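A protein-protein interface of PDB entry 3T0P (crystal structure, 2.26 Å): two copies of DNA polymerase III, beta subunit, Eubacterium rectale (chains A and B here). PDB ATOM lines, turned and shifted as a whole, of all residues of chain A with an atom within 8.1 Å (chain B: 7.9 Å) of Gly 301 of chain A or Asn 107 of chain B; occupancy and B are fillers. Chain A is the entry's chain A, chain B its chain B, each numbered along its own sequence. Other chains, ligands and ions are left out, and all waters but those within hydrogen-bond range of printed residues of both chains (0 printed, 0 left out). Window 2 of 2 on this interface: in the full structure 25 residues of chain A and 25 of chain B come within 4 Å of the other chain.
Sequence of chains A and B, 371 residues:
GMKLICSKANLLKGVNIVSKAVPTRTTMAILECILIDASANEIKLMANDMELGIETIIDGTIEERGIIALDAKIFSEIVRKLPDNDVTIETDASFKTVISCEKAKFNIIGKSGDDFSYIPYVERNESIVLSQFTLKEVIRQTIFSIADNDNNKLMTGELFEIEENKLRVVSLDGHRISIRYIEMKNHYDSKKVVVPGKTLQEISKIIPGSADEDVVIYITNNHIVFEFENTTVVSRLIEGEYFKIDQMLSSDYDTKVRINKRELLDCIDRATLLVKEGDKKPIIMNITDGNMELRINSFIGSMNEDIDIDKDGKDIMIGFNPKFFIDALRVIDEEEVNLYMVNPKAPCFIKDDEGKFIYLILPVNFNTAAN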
ATOM      1  N   ALA A 271     -17.315 -21.977 -18.227  1.00  0.00           N
ATOM      2  CA  ALA A 271     -18.153 -20.800 -18.406  1.00  0.00           C
ATOM      3  C   ALA A 271     -18.469 -20.512 -19.898  1.00  0.00           C
ATOM      4  O   ALA A 271     -19.586 -20.112 -20.201  1.00  0.00           O
ATOM      5  CB  ALA A 271     -17.471 -19.596 -17.791  1.00  0.00           C
ATOM      6  N   LEU A 273     -19.179 -22.462 -22.340  1.00  0.00           N
ATOM      7  CA  LEU A 273     -20.247 -23.262 -22.937  1.00  0.00           C
ATOM      8  C   LEU A 273     -21.614 -22.499 -22.857  1.00  0.00           C
ATOM      9  O   LEU A 273     -22.514 -22.777 -23.640  1.00  0.00           O
ATOM     10  CB  LEU A 273     -20.334 -24.672 -22.293  1.00  0.00           C
ATOM     11  CG  LEU A 273     -20.938 -24.834 -20.873  1.00  0.00           C
ATOM     12  CD1 LEU A 273     -22.456 -24.951 -20.913  1.00  0.00           C
ATOM     13  CD2 LEU A 273     -20.352 -26.046 -20.174  1.00  0.00           C
ATOM     14  N   LEU A 274     -21.754 -21.548 -21.921  1.00  0.00           N
ATOM     15  CA  LEU A 274     -23.003 -20.797 -21.780  1.00  0.00           C
ATOM     16  C   LEU A 274     -23.125 -19.620 -22.778  1.00  0.00           C
ATOM     17  O   LEU A 274     -24.211 -19.070 -22.916  1.00  0.00           O
ATOM     18  CB  LEU A 274     -23.168 -20.300 -20.345  1.00  0.00           C
ATOM     19  CG  LEU A 274     -23.428 -21.378 -19.308  1.00  0.00           C
ATOM     20  CD1 LEU A 274     -23.364 -20.814 -17.934  1.00  0.00           C
ATOM     21  CD2 LEU A 274     -24.788 -22.051 -19.510  1.00  0.00           C
ATOM     22  N   VAL A 275     -22.043 -19.254 -23.482  1.00  0.00           N
ATOM     23  CA  VAL A 275     -22.046 -18.159 -24.447  1.00  0.00           C
ATOM     24  C   VAL A 275     -21.889 -18.755 -25.872  1.00  0.00           C
ATOM     25  O   VAL A 275     -20.871 -19.374 -26.187  1.00  0.00           O
ATOM     26  CB  VAL A 275     -21.027 -17.018 -24.115  1.00  0.00           C
ATOM     27  CG1 VAL A 275     -21.331 -16.416 -22.756  1.00  0.00           C
ATOM     28  CG2 VAL A 275     -19.576 -17.481 -24.152  1.00  0.00           C
ATOM     29  N   ASP A 279     -23.960 -14.390 -28.847  1.00  0.00           N
ATOM     30  CA  ASP A 279     -23.746 -13.898 -27.490  1.00  0.00           C
ATOM     31  C   ASP A 279     -22.297 -13.507 -27.266  1.00  0.00           C
ATOM     32  O   ASP A 279     -21.379 -14.108 -27.833  1.00  0.00           O
ATOM     33  CB  ASP A 279     -24.171 -14.942 -26.430  1.00  0.00           C
ATOM     34  CG  ASP A 279     -25.171 -14.465 -25.395  1.00  0.00           C
ATOM     35  OD1 ASP A 279     -25.142 -13.256 -25.044  1.00  0.00           O
ATOM     36  OD2 ASP A 279     -25.947 -15.307 -24.890  1.00  0.00           O
ATOM     37  N   LYS A 281     -20.941 -12.425 -23.621  1.00  0.00           N
ATOM     38  CA  LYS A 281     -21.123 -12.111 -22.193  1.00  0.00           C
ATOM     39  C   LYS A 281     -19.790 -12.158 -21.413  1.00  0.00           C
ATOM     40  O   LYS A 281     -18.933 -12.969 -21.726  1.00  0.00           O
ATOM     41  CB  LYS A 281     -22.146 -13.055 -21.545  1.00  0.00           C
ATOM     42  CG  LYS A 281     -23.582 -12.834 -22.024  1.00  0.00           C
ATOM     43  CD  LYS A 281     -24.332 -11.786 -21.213  1.00  0.00           C
ATOM     44  CE  LYS A 281     -25.734 -11.583 -21.717  1.00  0.00           C
ATOM     45  NZ  LYS A 281     -26.750 -12.143 -20.783  1.00  0.00           N
ATOM     46  N   ILE A 296     -21.054 -16.305 -14.712  1.00  0.00           N
ATOM     47  CA  ILE A 296     -21.440 -15.981 -16.077  1.00  0.00           C
ATOM     48  C   ILE A 296     -22.954 -16.232 -16.166  1.00  0.00           C
ATOM     49  O   ILE A 296     -23.459 -17.100 -15.470  1.00  0.00           O
ATOM     50  CB  ILE A 296     -20.585 -16.711 -17.143  1.00  0.00           C
ATOM     51  CG1 ILE A 296     -20.676 -15.994 -18.513  1.00  0.00           C
ATOM     52  CG2 ILE A 296     -20.927 -18.209 -17.250  1.00  0.00           C
ATOM     53  CD1 ILE A 296     -19.523 -16.248 -19.477  1.00  0.00           C
ATOM     54  N   ASN A 297     -23.676 -15.388 -16.921  1.00  0.00           N
ATOM     55  CA  ASN A 297     -25.129 -15.427 -17.119  1.00  0.00           C
ATOM     56  C   ASN A 297     -25.496 -15.257 -18.571  1.00  0.00           C
ATOM     57  O   ASN A 297     -25.020 -14.315 -19.202  1.00  0.00           O
ATOM     58  CB  ASN A 297     -25.789 -14.314 -16.339  1.00  0.00           C
ATOM     59  CG  ASN A 297     -26.084 -14.677 -14.927  1.00  0.00           C
ATOM     60  OD1 ASN A 297     -27.168 -15.184 -14.615  1.00  0.00           O
ATOM     61  ND2 ASN A 297     -25.124 -14.425 -14.050  1.00  0.00           N
ATOM     62  N   SER A 298     -26.323 -16.154 -19.119  1.00  0.00           N
ATOM     63  CA  SER A 298     -26.799 -16.003 -20.494  1.00  0.00           C
ATOM     64  C   SER A 298     -28.239 -16.480 -20.579  1.00  0.00           C
ATOM     65  O   SER A 298     -28.832 -16.820 -19.549  1.00  0.00           O
ATOM     66  CB  SER A 298     -25.897 -16.730 -21.492  1.00  0.00           C
ATOM     67  OG  SER A 298     -26.038 -18.139 -21.440  1.00  0.00           O
ATOM     68  N   PHE A 299     -28.812 -16.500 -21.799  1.00  0.00           N
ATOM     69  CA  PHE A 299     -30.166 -17.008 -22.026  1.00  0.00           C
ATOM     70  C   PHE A 299     -30.200 -18.517 -21.763  1.00  0.00           C
ATOM     71  O   PHE A 299     -31.230 -19.027 -21.333  1.00  0.00           O
ATOM     72  CB  PHE A 299     -30.659 -16.680 -23.453  1.00  0.00           C
ATOM     73  CG  PHE A 299     -29.737 -17.137 -24.557  1.00  0.00           C
ATOM     74  N   ILE A 300     -29.064 -19.218 -21.983  1.00  0.00           N
ATOM     75  CA  ILE A 300     -28.930 -20.667 -21.761  1.00  0.00           C
ATOM     76  C   ILE A 300     -29.001 -21.008 -20.256  1.00  0.00           C
ATOM     77  O   ILE A 300     -29.604 -22.017 -19.896  1.00  0.00           O
ATOM     78  CB  ILE A 300     -27.637 -21.205 -22.401  1.00  0.00           C
ATOM     79  CG1 ILE A 300     -27.682 -21.027 -23.923  1.00  0.00           C
ATOM     80  CG2 ILE A 300     -27.426 -22.668 -22.044  1.00  0.00           C
ATOM     81  CD1 ILE A 300     -26.357 -21.121 -24.614  1.00  0.00           C
ATOM     82  N   GLY A 301     -28.397 -20.169 -19.414  1.00  0.00           N
ATOM     83  CA  GLY A 301     -28.382 -20.357 -17.968  1.00  0.00           C
ATOM     84  C   GLY A 301     -27.227 -19.652 -17.283  1.00  0.00           C
ATOM     85  O   GLY A 301     -26.635 -18.730 -17.834  1.00  0.00           O
ATOM     86  N   SER A 302     -26.899 -20.064 -16.079  1.00  0.00           N
ATOM     87  CA  SER A 302     -25.807 -19.421 -15.359  1.00  0.00           C
ATOM     88  C   SER A 302     -24.824 -20.442 -14.761  1.00  0.00           C
ATOM     89  O   SER A 302     -25.102 -21.634 -14.645  1.00  0.00           O
ATOM     90  CB  SER A 302     -26.359 -18.518 -14.256  1.00  0.00           C
ATOM     91  OG  SER A 302     -27.069 -19.281 -13.291  1.00  0.00           O
ATOM     92  N   MET A 303     -23.678 -19.942 -14.369  1.00  0.00           N
ATOM     93  CA  MET A 303     -22.651 -20.729 -13.722  1.00  0.00           C
ATOM     94  C   MET A 303     -22.094 -19.971 -12.543  1.00  0.00           C
ATOM     95  O   MET A 303     -21.906 -18.759 -12.622  1.00  0.00           O
ATOM     96  CB  MET A 303     -21.520 -21.062 -14.704  1.00  0.00           C
ATOM     97  CG  MET A 303     -20.559 -22.090 -14.141  1.00  0.00           C
ATOM     98  SD  MET A 303     -18.772 -22.044 -14.878  1.00  0.00           S
ATOM     99  CE  MET A 303     -18.299 -23.564 -13.974  1.00  0.00           C
ATOM    100  N   ASN A 304     -21.801 -20.681 -11.467  1.00  0.00           N
ATOM    101  CA  ASN A 304     -21.119 -20.131 -10.314  1.00  0.00           C
ATOM    102  C   ASN A 304     -19.994 -21.101  -9.918  1.00  0.00           C
ATOM    103  O   ASN A 304     -20.249 -22.303  -9.795  1.00  0.00           O
ATOM    104  CB  ASN A 304     -22.090 -19.888  -9.168  1.00  0.00           C
ATOM    105  CG  ASN A 304     -21.451 -19.089  -8.056  1.00  0.00           C
ATOM    106  OD1 ASN A 304     -21.379 -17.866  -8.124  1.00  0.00           O
ATOM    107  ND2 ASN A 304     -20.886 -19.762  -7.062  1.00  0.00           N
ATOM    108  N   ILE B  74     -26.120 -28.684 -24.577  1.00  0.00           N
ATOM    109  CA  ILE B  74     -25.718 -28.037 -23.328  1.00  0.00           C
ATOM    110  C   ILE B  74     -25.360 -29.084 -22.255  1.00  0.00           C
ATOM    111  O   ILE B  74     -24.315 -28.956 -21.636  1.00  0.00           O
ATOM    112  CB  ILE B  74     -26.786 -27.025 -22.819  1.00  0.00           C
ATOM    113  CG1 ILE B  74     -27.124 -25.953 -23.893  1.00  0.00           C
ATOM    114  CG2 ILE B  74     -26.367 -26.364 -21.495  1.00  0.00           C
ATOM    115  CD1 ILE B  74     -25.885 -25.238 -24.679  1.00  0.00           C
ATOM    116  N   ILE B  78     -21.681 -29.605 -20.629  1.00  0.00           N
ATOM    117  CA  ILE B  78     -21.531 -29.411 -19.182  1.00  0.00           C
ATOM    118  C   ILE B  78     -20.782 -30.613 -18.600  1.00  0.00           C
ATOM    119  O   ILE B  78     -19.748 -30.420 -17.979  1.00  0.00           O
ATOM    120  CB  ILE B  78     -22.877 -29.157 -18.452  1.00  0.00           C
ATOM    121  CG1 ILE B  78     -23.450 -27.776 -18.817  1.00  0.00           C
ATOM    122  CG2 ILE B  78     -22.738 -29.303 -16.924  1.00  0.00           C
ATOM    123  CD1 ILE B  78     -24.835 -27.452 -18.248  1.00  0.00           C
ATOM    124  N   GLU B  90     -29.997 -31.953  -9.823  1.00  0.00           N
ATOM    125  CA  GLU B  90     -31.180 -31.643  -9.053  1.00  0.00           C
ATOM    126  C   GLU B  90     -32.126 -30.775  -9.876  1.00  0.00           C
ATOM    127  O   GLU B  90     -31.696 -29.796 -10.486  1.00  0.00           O
ATOM    128  CB  GLU B  90     -30.792 -30.940  -7.750  1.00  0.00           C
ATOM    129  CG  GLU B  90     -31.925 -30.901  -6.740  1.00  0.00           C
ATOM    130  CD  GLU B  90     -31.541 -30.846  -5.272  1.00  0.00           C
ATOM    131  OE1 GLU B  90     -30.342 -30.644  -4.961  1.00  0.00           O
ATOM    132  OE2 GLU B  90     -32.453 -31.004  -4.427  1.00  0.00           O
ATOM    133  N   LYS B  96     -36.305 -26.068 -13.379  1.00  0.00           N
ATOM    134  CA  LYS B  96     -35.002 -25.452 -13.149  1.00  0.00           C
ATOM    135  C   LYS B  96     -34.079 -26.584 -12.681  1.00  0.00           C
ATOM    136  O   LYS B  96     -34.445 -27.364 -11.795  1.00  0.00           O
ATOM    137  CB  LYS B  96     -35.087 -24.300 -12.128  1.00  0.00           C
ATOM    138  N   THR B  97     -32.941 -26.733 -13.353  1.00  0.00           N
ATOM    139  CA  THR B  97     -31.994 -27.800 -13.099  1.00  0.00           C
ATOM    140  C   THR B  97     -30.658 -27.228 -12.639  1.00  0.00           C
ATOM    141  O   THR B  97     -30.090 -26.326 -13.271  1.00  0.00           O
ATOM    142  CB  THR B  97     -31.845 -28.663 -14.383  1.00  0.00           C
ATOM    143  OG1 THR B  97     -33.140 -29.124 -14.769  1.00  0.00           O
ATOM    144  CG2 THR B  97     -30.925 -29.882 -14.187  1.00  0.00           C
ATOM    145  N   VAL B  98     -30.143 -27.806 -11.550  1.00  0.00           N
ATOM    146  CA  VAL B  98     -28.822 -27.504 -11.004  1.00  0.00           C
ATOM    147  C   VAL B  98     -27.942 -28.730 -11.196  1.00  0.00           C
ATOM    148  O   VAL B  98     -28.303 -29.838 -10.792  1.00  0.00           O
ATOM    149  CB  VAL B  98     -28.830 -27.058  -9.522  1.00  0.00           C
ATOM    150  CG1 VAL B  98     -27.499 -26.409  -9.166  1.00  0.00           C
ATOM    151  CG2 VAL B  98     -29.991 -26.113  -9.235  1.00  0.00           C
ATOM    152  N   ILE B  99     -26.814 -28.533 -11.852  1.00  0.00           N
ATOM    153  CA  ILE B  99     -25.808 -29.558 -12.083  1.00  0.00           C
ATOM    154  C   ILE B  99     -24.594 -29.070 -11.319  1.00  0.00           C
ATOM    155  O   ILE B  99     -24.103 -27.967 -11.592  1.00  0.00           O
ATOM    156  CB  ILE B  99     -25.529 -29.807 -13.590  1.00  0.00           C
ATOM    157  CG1 ILE B  99     -26.840 -30.134 -14.360  1.00  0.00           C
ATOM    158  CG2 ILE B  99     -24.498 -30.914 -13.735  1.00  0.00           C
ATOM    159  CD1 ILE B  99     -26.724 -30.190 -15.920  1.00  0.00           C
ATOM    160  N   SER B 100     -24.158 -29.843 -10.323  1.00  0.00           N
ATOM    161  CA  SER B 100     -23.059 -29.404  -9.472  1.00  0.00           C
ATOM    162  C   SER B 100     -21.987 -30.482  -9.332  1.00  0.00           C
ATOM    163  O   SER B 100     -22.269 -31.668  -9.424  1.00  0.00           O
ATOM    164  CB  SER B 100     -23.573 -28.928  -8.111  1.00  0.00           C
ATOM    165  OG  SER B 100     -23.953 -30.012  -7.295  1.00  0.00           O
ATOM    166  N   LYS B 105     -21.036 -25.048 -10.226  1.00  0.00           N
ATOM    167  CA  LYS B 105     -22.480 -25.167 -10.256  1.00  0.00           C
ATOM    168  C   LYS B 105     -23.055 -24.528 -11.523  1.00  0.00           C
ATOM    169  O   LYS B 105     -22.678 -23.412 -11.867  1.00  0.00           O
ATOM    170  CB  LYS B 105     -23.010 -24.459  -8.985  1.00  0.00           C
ATOM    171  CG  LYS B 105     -24.450 -24.692  -8.629  1.00  0.00           C
ATOM    172  CD  LYS B 105     -24.764 -24.013  -7.299  1.00  0.00           C
ATOM    173  CE  LYS B 105     -25.730 -22.847  -7.404  1.00  0.00           C
ATOM    174  NZ  LYS B 105     -25.089 -21.624  -7.963  1.00  0.00           N
ATOM    175  N   PHE B 106     -23.943 -25.252 -12.225  1.00  0.00           N
ATOM    176  CA  PHE B 106     -24.627 -24.770 -13.424  1.00  0.00           C
ATOM    177  C   PHE B 106     -26.107 -24.709 -13.185  1.00  0.00           C
ATOM    178  O   PHE B 106     -26.674 -25.677 -12.683  1.00  0.00           O
ATOM    179  CB  PHE B 106     -24.365 -25.676 -14.638  1.00  0.00           C
ATOM    180  CG  PHE B 106     -23.021 -25.475 -15.276  1.00  0.00           C
ATOM    181  CD1 PHE B 106     -22.841 -24.508 -16.257  1.00  0.00           C
ATOM    182  CD2 PHE B 106     -21.923 -26.227 -14.870  1.00  0.00           C
ATOM    183  CE1 PHE B 106     -21.595 -24.306 -16.826  1.00  0.00           C
ATOM    184  CE2 PHE B 106     -20.673 -26.026 -15.442  1.00  0.00           C
ATOM    185  CZ  PHE B 106     -20.521 -25.086 -16.438  1.00  0.00           C
ATOM    186  N   ASN B 107     -26.752 -23.594 -13.544  1.00  0.00           N
ATOM    187  CA  ASN B 107     -28.214 -23.496 -13.465  1.00  0.00           C
ATOM    188  C   ASN B 107     -28.727 -23.417 -14.882  1.00  0.00           C
ATOM    189  O   ASN B 107     -28.284 -22.552 -15.649  1.00  0.00           O
ATOM    190  CB  ASN B 107     -28.678 -22.317 -12.620  1.00  0.00           C
ATOM    191  CG  ASN B 107     -28.172 -22.373 -11.205  1.00  0.00           C
ATOM    192  OD1 ASN B 107     -28.798 -22.964 -10.326  1.00  0.00           O
ATOM    193  ND2 ASN B 107     -26.992 -21.814 -10.970  1.00  0.00           N
ATOM    194  N   ILE B 108     -29.543 -24.415 -15.282  1.00  0.00           N
ATOM    195  CA  ILE B 108     -30.148 -24.470 -16.612  1.00  0.00           C
ATOM    196  C   ILE B 108     -31.638 -24.772 -16.432  1.00  0.00           C
ATOM    197  O   ILE B 108     -32.088 -24.984 -15.308  1.00  0.00           O
ATOM    198  CB  ILE B 108     -29.438 -25.451 -17.607  1.00  0.00           C
ATOM    199  CG1 ILE B 108     -29.422 -26.914 -17.083  1.00  0.00           C
ATOM    200  CG2 ILE B 108     -28.036 -24.933 -18.007  1.00  0.00           C
ATOM    201  CD1 ILE B 108     -28.931 -27.931 -18.061  1.00  0.00           C
ATOM    202  N   ILE B 109     -32.396 -24.747 -17.529  1.00  0.00           N
ATOM    203  CA  ILE B 109     -33.824 -25.025 -17.511  1.00  0.00           C
ATOM    204  C   ILE B 109     -34.073 -26.271 -18.366  1.00  0.00           C
ATOM    205  O   ILE B 109     -33.603 -26.349 -19.503  1.00  0.00           O
ATOM    206  CB  ILE B 109     -34.690 -23.798 -17.941  1.00  0.00           C
ATOM    207  CG1 ILE B 109     -34.183 -23.130 -19.247  1.00  0.00           C
ATOM    208  CG2 ILE B 109     -34.803 -22.767 -16.804  1.00  0.00           C
ATOM    209  N   GLY B 110     -34.762 -27.240 -17.789  1.00  0.00           N
ATOM    210  CA  GLY B 110     -35.112 -28.470 -18.476  1.00  0.00           C
ATOM    211  C   GLY B 110     -36.529 -28.402 -18.999  1.00  0.00           C
ATOM    212  O   GLY B 110     -37.168 -27.346 -18.975  1.00  0.00           O
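Among the printed residues, merely in contact across the chains: Leu 273 of chain A with Ile 78 of chain B, Leu 273 of chain A with Phe 106 of chain B, Ile 300 of chain A with Ile 74 of chain B, Ile 300 of chain A with Ile 108 of chain B, Gly 301 of chain A with Asn 107 of chain B, Ser 302 of chain A with Phe 106 of chain B, Met 303 of chain A with Lys 105 of chain B and Met 303 of chain A with Phe 106 of chain B.
Of the 15 printed residues of chain A, 6 touch a printed residue of chain B.
Of the 14 printed residues of chain B, 6 touch a printed residue of chain A.
Printed residues of chain B that touch a printed residue of chain A: Ile 74, Ile 78, Lys 105, Phe 106, Asn 107 and Ile 108.
Hydrophobic or aromatic side chains of chain B within 4 Å of the printed part of chain A: Ile 74, Ile 78, Phe 106 and Ile 108.
Of chain B, only Asn 107 comes within 4 Å of Gly 301 of chain A.
Asn 107 of chain B touches two residues of chain A.
Of chain B, only Phe 106 and Asn 107 come within 4 Å of Ser 302 of chain A.
Printed residues of chain B within 4 Å of Leu 273 of chain A: Ile 78 (3.7 Å) and Phe 106 (3.9 Å).
Printed residues of chain B within 4 Å of Met 303 of chain A: Lys 105 (3.3 Å) and Phe 106 (3.6 Å).
Of the printed residues of chain A, Ile 108 of chain B touches Ile 300.
Of the printed residues of chain A, Lys 105 of chain B touches Met 303 and Asn 304.
Of the printed residues of chain A, Ile 78 of chain B touches Leu 273.
Val 275 of chain A touches none of the printed residues of chain B.
The nearest residue of chain A that does not touch Asn 107 of chain B is Ile 300 of chain A (4.5 Å).
The nearest printed residue of chain A that does not touch Lys 105 of chain B is Ser 302 of chain A (4.1 Å).
N of Ala 271 of chain A lies within hydrogen-bond range of SD of Met 303 of chain A, 3.7 Å away.
The backbone carbonyl oxygen (O) of Ile 296 of chain A is in hydrogen-bond range of the backbone NH (N) of Met 303 of chain A (3.1 Å).
The backbone NH (N) of Ile 300 of chain A lies close to the side-chain hydroxyl (OG) of Ser 298 of chain A (3.3 Å).
The backbone NH (N) of Thr 97 of chain B sits at hydrogen-bond distance from the backbone carbonyl oxygen (O) of Ile 108 of chain B.
O of Ile 99 of chain B lies within hydrogen-bond range of N of Phe 106 of chain B, 2.8 Å away.
The backbone NH of Asn 107 of chain B lies within hydrogen-bond range of the backbone carbonyl oxygen of Ser 302 of chain A.
The backbone carbonyl oxygen (O) of Asn 304 of chain A lies within hydrogen-bond range of the backbone NH (N) of Lys 105 of chain B, 2.9 Å away.
No position is printed for both chains.
Of the 10 pairs that touch across the chains among the printed residues, none has its exchanged pair printed and touching as well.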
